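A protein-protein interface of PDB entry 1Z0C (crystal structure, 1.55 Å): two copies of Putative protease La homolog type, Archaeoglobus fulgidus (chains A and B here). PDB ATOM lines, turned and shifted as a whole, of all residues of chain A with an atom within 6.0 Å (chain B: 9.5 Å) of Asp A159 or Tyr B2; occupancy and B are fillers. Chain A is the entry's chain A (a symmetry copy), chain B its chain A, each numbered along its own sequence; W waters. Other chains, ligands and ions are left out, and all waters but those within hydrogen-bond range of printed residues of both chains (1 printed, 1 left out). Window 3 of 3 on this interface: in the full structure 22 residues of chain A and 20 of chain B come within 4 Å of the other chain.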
ATOM      1  N   PRO A 131     -30.817 -26.162  13.425  1.00  0.00           N
ATOM      2  CA  PRO A 131     -29.993 -26.756  14.458  1.00  0.00           C
ATOM      3  C   PRO A 131     -29.102 -25.740  15.139  1.00  0.00           C
ATOM      4  O   PRO A 131     -28.785 -24.686  14.568  1.00  0.00           O
ATOM      5  CB  PRO A 131     -29.156 -27.804  13.694  1.00  0.00           C
ATOM      6  CG  PRO A 131     -29.248 -27.444  12.300  1.00  0.00           C
ATOM      7  CD  PRO A 131     -30.453 -26.585  12.060  1.00  0.00           C
ATOM      8  N   VAL A 132     -28.751 -26.050  16.384  1.00  0.00           N
ATOM      9  CA  VAL A 132     -27.981 -25.209  17.258  1.00  0.00           C
ATOM     10  C   VAL A 132     -26.906 -26.043  17.966  1.00  0.00           C
ATOM     11  O   VAL A 132     -26.969 -27.268  17.966  1.00  0.00           O
ATOM     12  CB  VAL A 132     -28.885 -24.543  18.328  1.00  0.00           C
ATOM     13  CG1 VAL A 132     -29.898 -23.731  17.620  1.00  0.00           C
ATOM     14  CG2 VAL A 132     -29.604 -25.593  19.127  1.00  0.00           C
ATOM     15  N   GLY A 133     -25.986 -25.354  18.618  1.00  0.00           N
ATOM     16  CA  GLY A 133     -24.903 -26.030  19.344  1.00  0.00           C
ATOM     17  C   GLY A 133     -25.271 -26.317  20.790  1.00  0.00           C
ATOM     18  O   GLY A 133     -26.293 -25.830  21.322  1.00  0.00           O
ATOM     19  N   GLY A 134     -24.419 -27.107  21.431  1.00  0.00           N
ATOM     20  CA  GLY A 134     -24.496 -27.371  22.842  1.00  0.00           C
ATOM     21  C   GLY A 134     -25.752 -28.086  23.315  1.00  0.00           C
ATOM     22  O   GLY A 134     -26.144 -27.926  24.472  1.00  0.00           O
ATOM     23  N   VAL A 135     -26.374 -28.865  22.429  1.00  0.00           N
ATOM     24  CA  VAL A 135     -27.633 -29.546  22.782  1.00  0.00           C
ATOM     25  C   VAL A 135     -27.500 -30.492  23.995  1.00  0.00           C
ATOM     26  O   VAL A 135     -28.384 -30.545  24.836  1.00  0.00           O
ATOM     27  CB  VAL A 135     -28.365 -30.126  21.552  1.00  0.00           C
ATOM     28  CG1 VAL A 135     -29.545 -30.948  21.970  1.00  0.00           C
ATOM     29  CG2 VAL A 135     -28.857 -28.973  20.694  1.00  0.00           C
ATOM     30  N   THR A 136     -26.385 -31.211  24.137  1.00  0.00           N
ATOM     31  CA  THR A 136     -26.269 -32.109  25.296  1.00  0.00           C
ATOM     32  C   THR A 136     -26.237 -31.323  26.599  1.00  0.00           C
ATOM     33  O   THR A 136     -26.954 -31.626  27.545  1.00  0.00           O
ATOM     34  CB  THR A 136     -24.993 -32.943  25.207  1.00  0.00           C
ATOM     35  OG1 THR A 136     -24.955 -33.567  23.935  1.00  0.00           O
ATOM     36  CG2 THR A 136     -24.983 -33.992  26.300  1.00  0.00           C
ATOM     37  N   ASP A 155     -32.469 -31.847  13.553  1.00  0.00           N
ATOM     38  CA  ASP A 155     -31.114 -32.057  13.032  1.00  0.00           C
ATOM     39  C   ASP A 155     -30.090 -32.221  14.129  1.00  0.00           C
ATOM     40  O   ASP A 155     -28.933 -32.568  13.835  1.00  0.00           O
ATOM     41  CB  ASP A 155     -30.689 -30.936  12.080  1.00  0.00           C
ATOM     42  CG  ASP A 155     -31.122 -31.174  10.666  1.00  0.00           C
ATOM     43  OD1 ASP A 155     -32.027 -31.997  10.425  1.00  0.00           O
ATOM     44  OD2 ASP A 155     -30.529 -30.528   9.775  1.00  0.00           O
ATOM     45  N   ASN A 156     -30.517 -32.058  15.390  1.00  0.00           N
ATOM     46  CA  ASN A 156     -29.655 -32.175  16.567  1.00  0.00           C
ATOM     47  C   ASN A 156     -29.892 -33.437  17.399  1.00  0.00           C
ATOM     48  O   ASN A 156     -29.298 -33.573  18.478  1.00  0.00           O
ATOM     49  CB  ASN A 156     -29.795 -30.976  17.531  1.00  0.00           C
ATOM     50  CG  ASN A 156     -29.149 -29.673  17.012  1.00  0.00           C
ATOM     51  OD1 ASN A 156     -29.787 -28.626  17.031  1.00  0.00           O
ATOM     52  ND2 ASN A 156     -27.901 -29.733  16.544  1.00  0.00           N
ATOM     53  N   ILE A 157     -30.788 -34.300  16.944  1.00  0.00           N
ATOM     54  CA  ILE A 157     -31.111 -35.535  17.645  1.00  0.00           C
ATOM     55  C   ILE A 157     -29.851 -36.407  17.762  1.00  0.00           C
ATOM     56  O   ILE A 157     -29.657 -37.042  18.793  1.00  0.00           O
ATOM     57  CB  ILE A 157     -32.196 -36.393  16.950  1.00  0.00           C
ATOM     58  CG1 ILE A 157     -33.539 -35.661  16.845  1.00  0.00           C
ATOM     59  CG2 ILE A 157     -32.376 -37.721  17.719  1.00  0.00           C
ATOM     60  CD1 ILE A 157     -34.386 -36.166  15.636  1.00  0.00           C
ATOM     61  N   ASP A 158     -28.986 -36.408  16.743  1.00  0.00           N
ATOM     62  CA  ASP A 158     -27.732 -37.211  16.792  1.00  0.00           C
ATOM     63  C   ASP A 158     -26.769 -36.573  17.791  1.00  0.00           C
ATOM     64  O   ASP A 158     -25.793 -37.183  18.245  1.00  0.00           O
ATOM     65  CB  ASP A 158     -27.029 -37.280  15.424  1.00  0.00           C
ATOM     66  CG  ASP A 158     -27.944 -37.754  14.284  1.00  0.00           C
ATOM     67  OD1 ASP A 158     -27.575 -37.514  13.089  1.00  0.00           O
ATOM     68  OD2 ASP A 158     -29.017 -38.349  14.556  1.00  0.00           O
ATOM     69  N   ASP A 159     -27.064 -35.333  18.140  1.00  0.00           N
ATOM     70  CA  ASP A 159     -26.145 -34.534  18.916  1.00  0.00           C
ATOM     71  C   ASP A 159     -26.337 -34.666  20.433  1.00  0.00           C
ATOM     72  O   ASP A 159     -25.570 -34.103  21.214  1.00  0.00           O
ATOM     73  CB  ASP A 159     -26.176 -33.085  18.403  1.00  0.00           C
ATOM     74  CG  ASP A 159     -25.790 -32.989  16.917  1.00  0.00           C
ATOM     75  OD1 ASP A 159     -24.892 -33.756  16.487  1.00  0.00           O
ATOM     76  OD2 ASP A 159     -26.350 -32.157  16.171  1.00  0.00           O
ATOM     77  N   VAL A 160     -27.320 -35.473  20.834  1.00  0.00           N
ATOM     78  CA  VAL A 160     -27.591 -35.740  22.248  1.00  0.00           C
ATOM     79  C   VAL A 160     -26.692 -36.856  22.819  1.00  0.00           C
ATOM     80  O   VAL A 160     -26.984 -38.051  22.641  1.00  0.00           O
ATOM     81  CB  VAL A 160     -29.065 -36.143  22.478  1.00  0.00           C
ATOM     82  CG1 VAL A 160     -29.352 -36.242  23.981  1.00  0.00           C
ATOM     83  CG2 VAL A 160     -30.024 -35.139  21.826  1.00  0.00           C
ATOM     84  N   LEU A 161     -25.613 -36.466  23.507  1.00  0.00           N
ATOM     85  CA  LEU A 161     -24.671 -37.430  24.122  1.00  0.00           C
ATOM     86  C   LEU A 161     -24.924 -37.525  25.631  1.00  0.00           C
ATOM     87  O   LEU A 161     -24.153 -37.038  26.467  1.00  0.00           O
ATOM     88  CB  LEU A 161     -23.205 -37.083  23.806  1.00  0.00           C
ATOM     89  CG  LEU A 161     -22.737 -36.757  22.378  1.00  0.00           C
ATOM     90  CD1 LEU A 161     -23.632 -37.317  21.254  1.00  0.00           C
ATOM     91  CD2 LEU A 161     -22.577 -35.257  22.221  1.00  0.00           C
ATOM     92  N   TYR B   2     -23.786 -30.812  13.323  1.00  0.00           N
ATOM     93  CA  TYR B   2     -24.850 -30.139  12.499  1.00  0.00           C
ATOM     94  C   TYR B   2     -24.181 -29.181  11.535  1.00  0.00           C
ATOM     95  O   TYR B   2     -22.986 -28.932  11.634  1.00  0.00           O
ATOM     96  CB  TYR B   2     -25.893 -29.399  13.389  1.00  0.00           C
ATOM     97  CG  TYR B   2     -25.304 -28.249  14.190  1.00  0.00           C
ATOM     98  CD1 TYR B   2     -24.561 -28.492  15.349  1.00  0.00           C
ATOM     99  CD2 TYR B   2     -25.454 -26.928  13.768  1.00  0.00           C
ATOM    100  CE1 TYR B   2     -23.990 -27.457  16.071  1.00  0.00           C
ATOM    101  CE2 TYR B   2     -24.900 -25.874  14.495  1.00  0.00           C
ATOM    102  CZ  TYR B   2     -24.142 -26.155  15.637  1.00  0.00           C
ATOM    103  OH  TYR B   2     -23.567 -25.132  16.380  1.00  0.00           O
ATOM    104  N   LYS B   3     -24.961 -28.671  10.593  1.00  0.00           N
ATOM    105  CA  LYS B   3     -24.468 -27.687   9.651  1.00  0.00           C
ATOM    106  C   LYS B   3     -25.492 -26.599   9.598  1.00  0.00           C
ATOM    107  O   LYS B   3     -26.684 -26.858   9.776  1.00  0.00           O
ATOM    108  CB  LYS B   3     -24.352 -28.306   8.262  1.00  0.00           C
ATOM    109  CG  LYS B   3     -22.993 -28.817   7.936  1.00  0.00           C
ATOM    110  CD  LYS B   3     -23.008 -29.527   6.590  1.00  0.00           C
ATOM    111  CE  LYS B   3     -21.619 -30.115   6.248  1.00  0.00           C
ATOM    112  NZ  LYS B   3     -21.354 -30.158   4.760  1.00  0.00           N
ATOM    113  N   LEU B   4     -25.044 -25.396   9.286  1.00  0.00           N
ATOM    114  CA  LEU B   4     -25.965 -24.287   9.166  1.00  0.00           C
ATOM    115  C   LEU B   4     -26.537 -24.137   7.748  1.00  0.00           C
ATOM    116  O   LEU B   4     -27.576 -23.500   7.558  1.00  0.00           O
ATOM    117  CB  LEU B   4     -25.339 -22.994   9.730  1.00  0.00           C
ATOM    118  CG  LEU B   4     -25.106 -23.061  11.257  1.00  0.00           C
ATOM    119  CD1 LEU B   4     -24.934 -21.697  11.826  1.00  0.00           C
ATOM    120  CD2 LEU B   4     -26.258 -23.762  11.984  1.00  0.00           C
ATOM    121  N   PHE B   5     -25.870 -24.774   6.786  1.00  0.00           N
ATOM    122  CA  PHE B   5     -26.327 -24.798   5.398  1.00  0.00           C
ATOM    123  C   PHE B   5     -26.838 -26.164   4.949  1.00  0.00           C
ATOM    124  O   PHE B   5     -26.486 -27.206   5.513  1.00  0.00           O
ATOM    125  CB  PHE B   5     -25.219 -24.327   4.456  1.00  0.00           C
ATOM    126  CG  PHE B   5     -23.876 -24.904   4.757  1.00  0.00           C
ATOM    127  CD1 PHE B   5     -23.393 -26.006   4.047  1.00  0.00           C
ATOM    128  CD2 PHE B   5     -23.069 -24.336   5.749  1.00  0.00           C
ATOM    129  CE1 PHE B   5     -22.122 -26.558   4.325  1.00  0.00           C
ATOM    130  CE2 PHE B   5     -21.798 -24.858   6.031  1.00  0.00           C
ATOM    131  CZ  PHE B   5     -21.321 -25.985   5.319  1.00  0.00           C
ATOM    132  N   ILE B   6     -27.700 -26.131   3.947  1.00  0.00           N
ATOM    133  CA  ILE B   6     -28.196 -27.330   3.296  1.00  0.00           C
ATOM    134  C   ILE B   6     -27.343 -27.481   2.045  1.00  0.00           C
ATOM    135  O   ILE B   6     -26.970 -26.476   1.416  1.00  0.00           O
ATOM    136  CB  ILE B   6     -29.671 -27.172   2.896  1.00  0.00           C
ATOM    137  CG1 ILE B   6     -30.564 -26.827   4.111  1.00  0.00           C
ATOM    138  CG2 ILE B   6     -30.125 -28.413   2.177  1.00  0.00           C
ATOM    139  CD1 ILE B   6     -32.052 -26.642   3.780  1.00  0.00           C
ATOM    140  N   ARG B  14     -34.049 -19.766   0.051  1.00  0.00           N
ATOM    141  CA  ARG B  14     -32.780 -20.014   0.771  1.00  0.00           C
ATOM    142  C   ARG B  14     -31.685 -20.147  -0.281  1.00  0.00           C
ATOM    143  O   ARG B  14     -31.842 -20.841  -1.284  1.00  0.00           O
ATOM    144  CB  ARG B  14     -32.828 -21.331   1.563  1.00  0.00           C
ATOM    145  CG  ARG B  14     -31.656 -21.500   2.431  1.00  0.00           C
ATOM    146  CD  ARG B  14     -31.993 -22.503   3.608  1.00  0.00           C
ATOM    147  NE  ARG B  14     -30.803 -22.778   4.395  1.00  0.00           N
ATOM    148  CZ  ARG B  14     -30.823 -23.321   5.603  1.00  0.00           C
ATOM    149  NH1 ARG B  14     -31.979 -23.697   6.133  1.00  0.00           N
ATOM    150  NH2 ARG B  14     -29.686 -23.537   6.254  1.00  0.00           N
ATOM    151  N   VAL B  85     -27.821 -16.971   8.223  1.00  0.00           N
ATOM    152  CA  VAL B  85     -27.710 -18.094   9.125  1.00  0.00           C
ATOM    153  C   VAL B  85     -26.266 -18.246   9.616  1.00  0.00           C
ATOM    154  O   VAL B  85     -25.330 -18.290   8.813  1.00  0.00           O
ATOM    155  CB  VAL B  85     -28.230 -19.398   8.487  1.00  0.00           C
ATOM    156  CG1 VAL B  85     -28.499 -20.394   9.546  1.00  0.00           C
ATOM    157  CG2 VAL B  85     -29.502 -19.159   7.724  1.00  0.00           C
ATOM    158  N   GLY B  86     -26.120 -18.263  10.946  1.00  0.00           N
ATOM    159  CA  GLY B  86     -24.811 -18.233  11.591  1.00  0.00           C
ATOM    160  C   GLY B  86     -24.298 -16.811  11.689  1.00  0.00           C
ATOM    161  O   GLY B  86     -24.063 -16.138  10.669  1.00  0.00           O
ATOM    162  N   THR B  87     -24.123 -16.360  12.926  1.00  0.00           N
ATOM    163  CA  THR B  87     -23.679 -15.006  13.214  1.00  0.00           C
ATOM    164  C   THR B  87     -22.186 -14.987  13.528  1.00  0.00           C
ATOM    165  O   THR B  87     -21.778 -15.268  14.657  1.00  0.00           O
ATOM    166  CB  THR B  87     -24.482 -14.430  14.402  1.00  0.00           C
ATOM    167  OG1 THR B  87     -25.890 -14.485  14.107  1.00  0.00           O
ATOM    168  CG2 THR B  87     -24.046 -12.986  14.727  1.00  0.00           C
ATOM    169  N   TYR B  88     -21.376 -14.652  12.528  1.00  0.00           N
ATOM    170  CA  TYR B  88     -19.919 -14.656  12.685  1.00  0.00           C
ATOM    171  C   TYR B  88     -19.370 -13.238  12.805  1.00  0.00           C
ATOM    172  O   TYR B  88     -19.826 -12.312  12.123  1.00  0.00           O
ATOM    173  CB  TYR B  88     -19.252 -15.383  11.516  1.00  0.00           C
ATOM    174  CG  TYR B  88     -19.438 -16.887  11.515  1.00  0.00           C
ATOM    175  CD1 TYR B  88     -20.718 -17.466  11.483  1.00  0.00           C
ATOM    176  CD2 TYR B  88     -18.334 -17.734  11.524  1.00  0.00           C
ATOM    177  CE1 TYR B  88     -20.880 -18.853  11.482  1.00  0.00           C
ATOM    178  CE2 TYR B  88     -18.487 -19.118  11.516  1.00  0.00           C
ATOM    179  CZ  TYR B  88     -19.757 -19.672  11.494  1.00  0.00           C
ATOM    180  OH  TYR B  88     -19.882 -21.049  11.488  1.00  0.00           O
HETATM  181  O   HOH W   1     -27.478 -30.317  10.067  1.00  0.00           O
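Printed residues of chain B that touch a printed residue of chain A: Tyr B2, Lys B3 and Leu B4. Hydrophobic or aromatic side chains of chain B within 4 Å of the printed part of chain A: Tyr B2 and Leu B4. Hydrophobic or aromatic side chains of chain A within 4 Å of the printed part of chain B: Pro A131.
The side-chain hydroxyl (OH) of Tyr B2 lies within hydrogen-bond range of the backbone NH (N) of Gly A133, at 3.3 Å.
Of chain B, only Tyr B2 (3.9 Å) comes within 4 Å of Asp A159. Tyr B2 touches just these residues of chain A: Pro A131, Val A132, Gly A133, Asn A156 and Asp A159. Pro A131 touches just these residues of chain B: Tyr B2 (3.6 Å), Lys B3 (3.6 Å) and Leu B4 (3.7 Å). No residue of chain B comes within 4 Å of Val A160. Printed residues of chain B within 4 Å of Gly A133: Tyr B2 (3.3 Å). Printed residues of chain B within 4 Å of Val A132: Tyr B2. Of the printed residues of chain A, Lys B3 touches Pro A131 (3.6 Å). Of the printed residues of chain A, Leu B4 touches Pro A131. The nearest printed residue of chain B that does not touch Val A132 is Leu B4 (5.6 Å).
Among the printed residues, pairs that only touch across the chains: Val A132 with Tyr B2 (3.5 Å), Pro A131 with Tyr B2 (3.6 Å), Pro A131 with Lys B3 (3.6 Å), Pro A131 with Leu B4 (3.7 Å), Asn A156 with Tyr B2 (3.8 Å) and Asp A159 with Tyr B2 (3.9 Å).
Water W1 lies within hydrogen-bond range of N of Lys B3 (3.1 Å) and OD2 of Asp A155 (3.1 Å).
No position is printed for both chains. Of the 7 pairs that touch across the chains among the printed residues, none has its exchanged pair printed and touching as well.
The guanidinium group (NH2) of Arg B14 is in hydrogen-bond range of the backbone carbonyl oxygen (O) of Leu B4, at 2.5 Å. The side-chain amide oxygen (OD1) of Asn A156 is in hydrogen-bond range of the backbone NH (N) of Val A132 (2.9 Å). OG1 of Thr A136 lies within hydrogen-bond range of O of Asp A159. ND2 of Asn A156 sits at hydrogen-bond distance from OD2 of Asp A159, 2.9 Å away.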
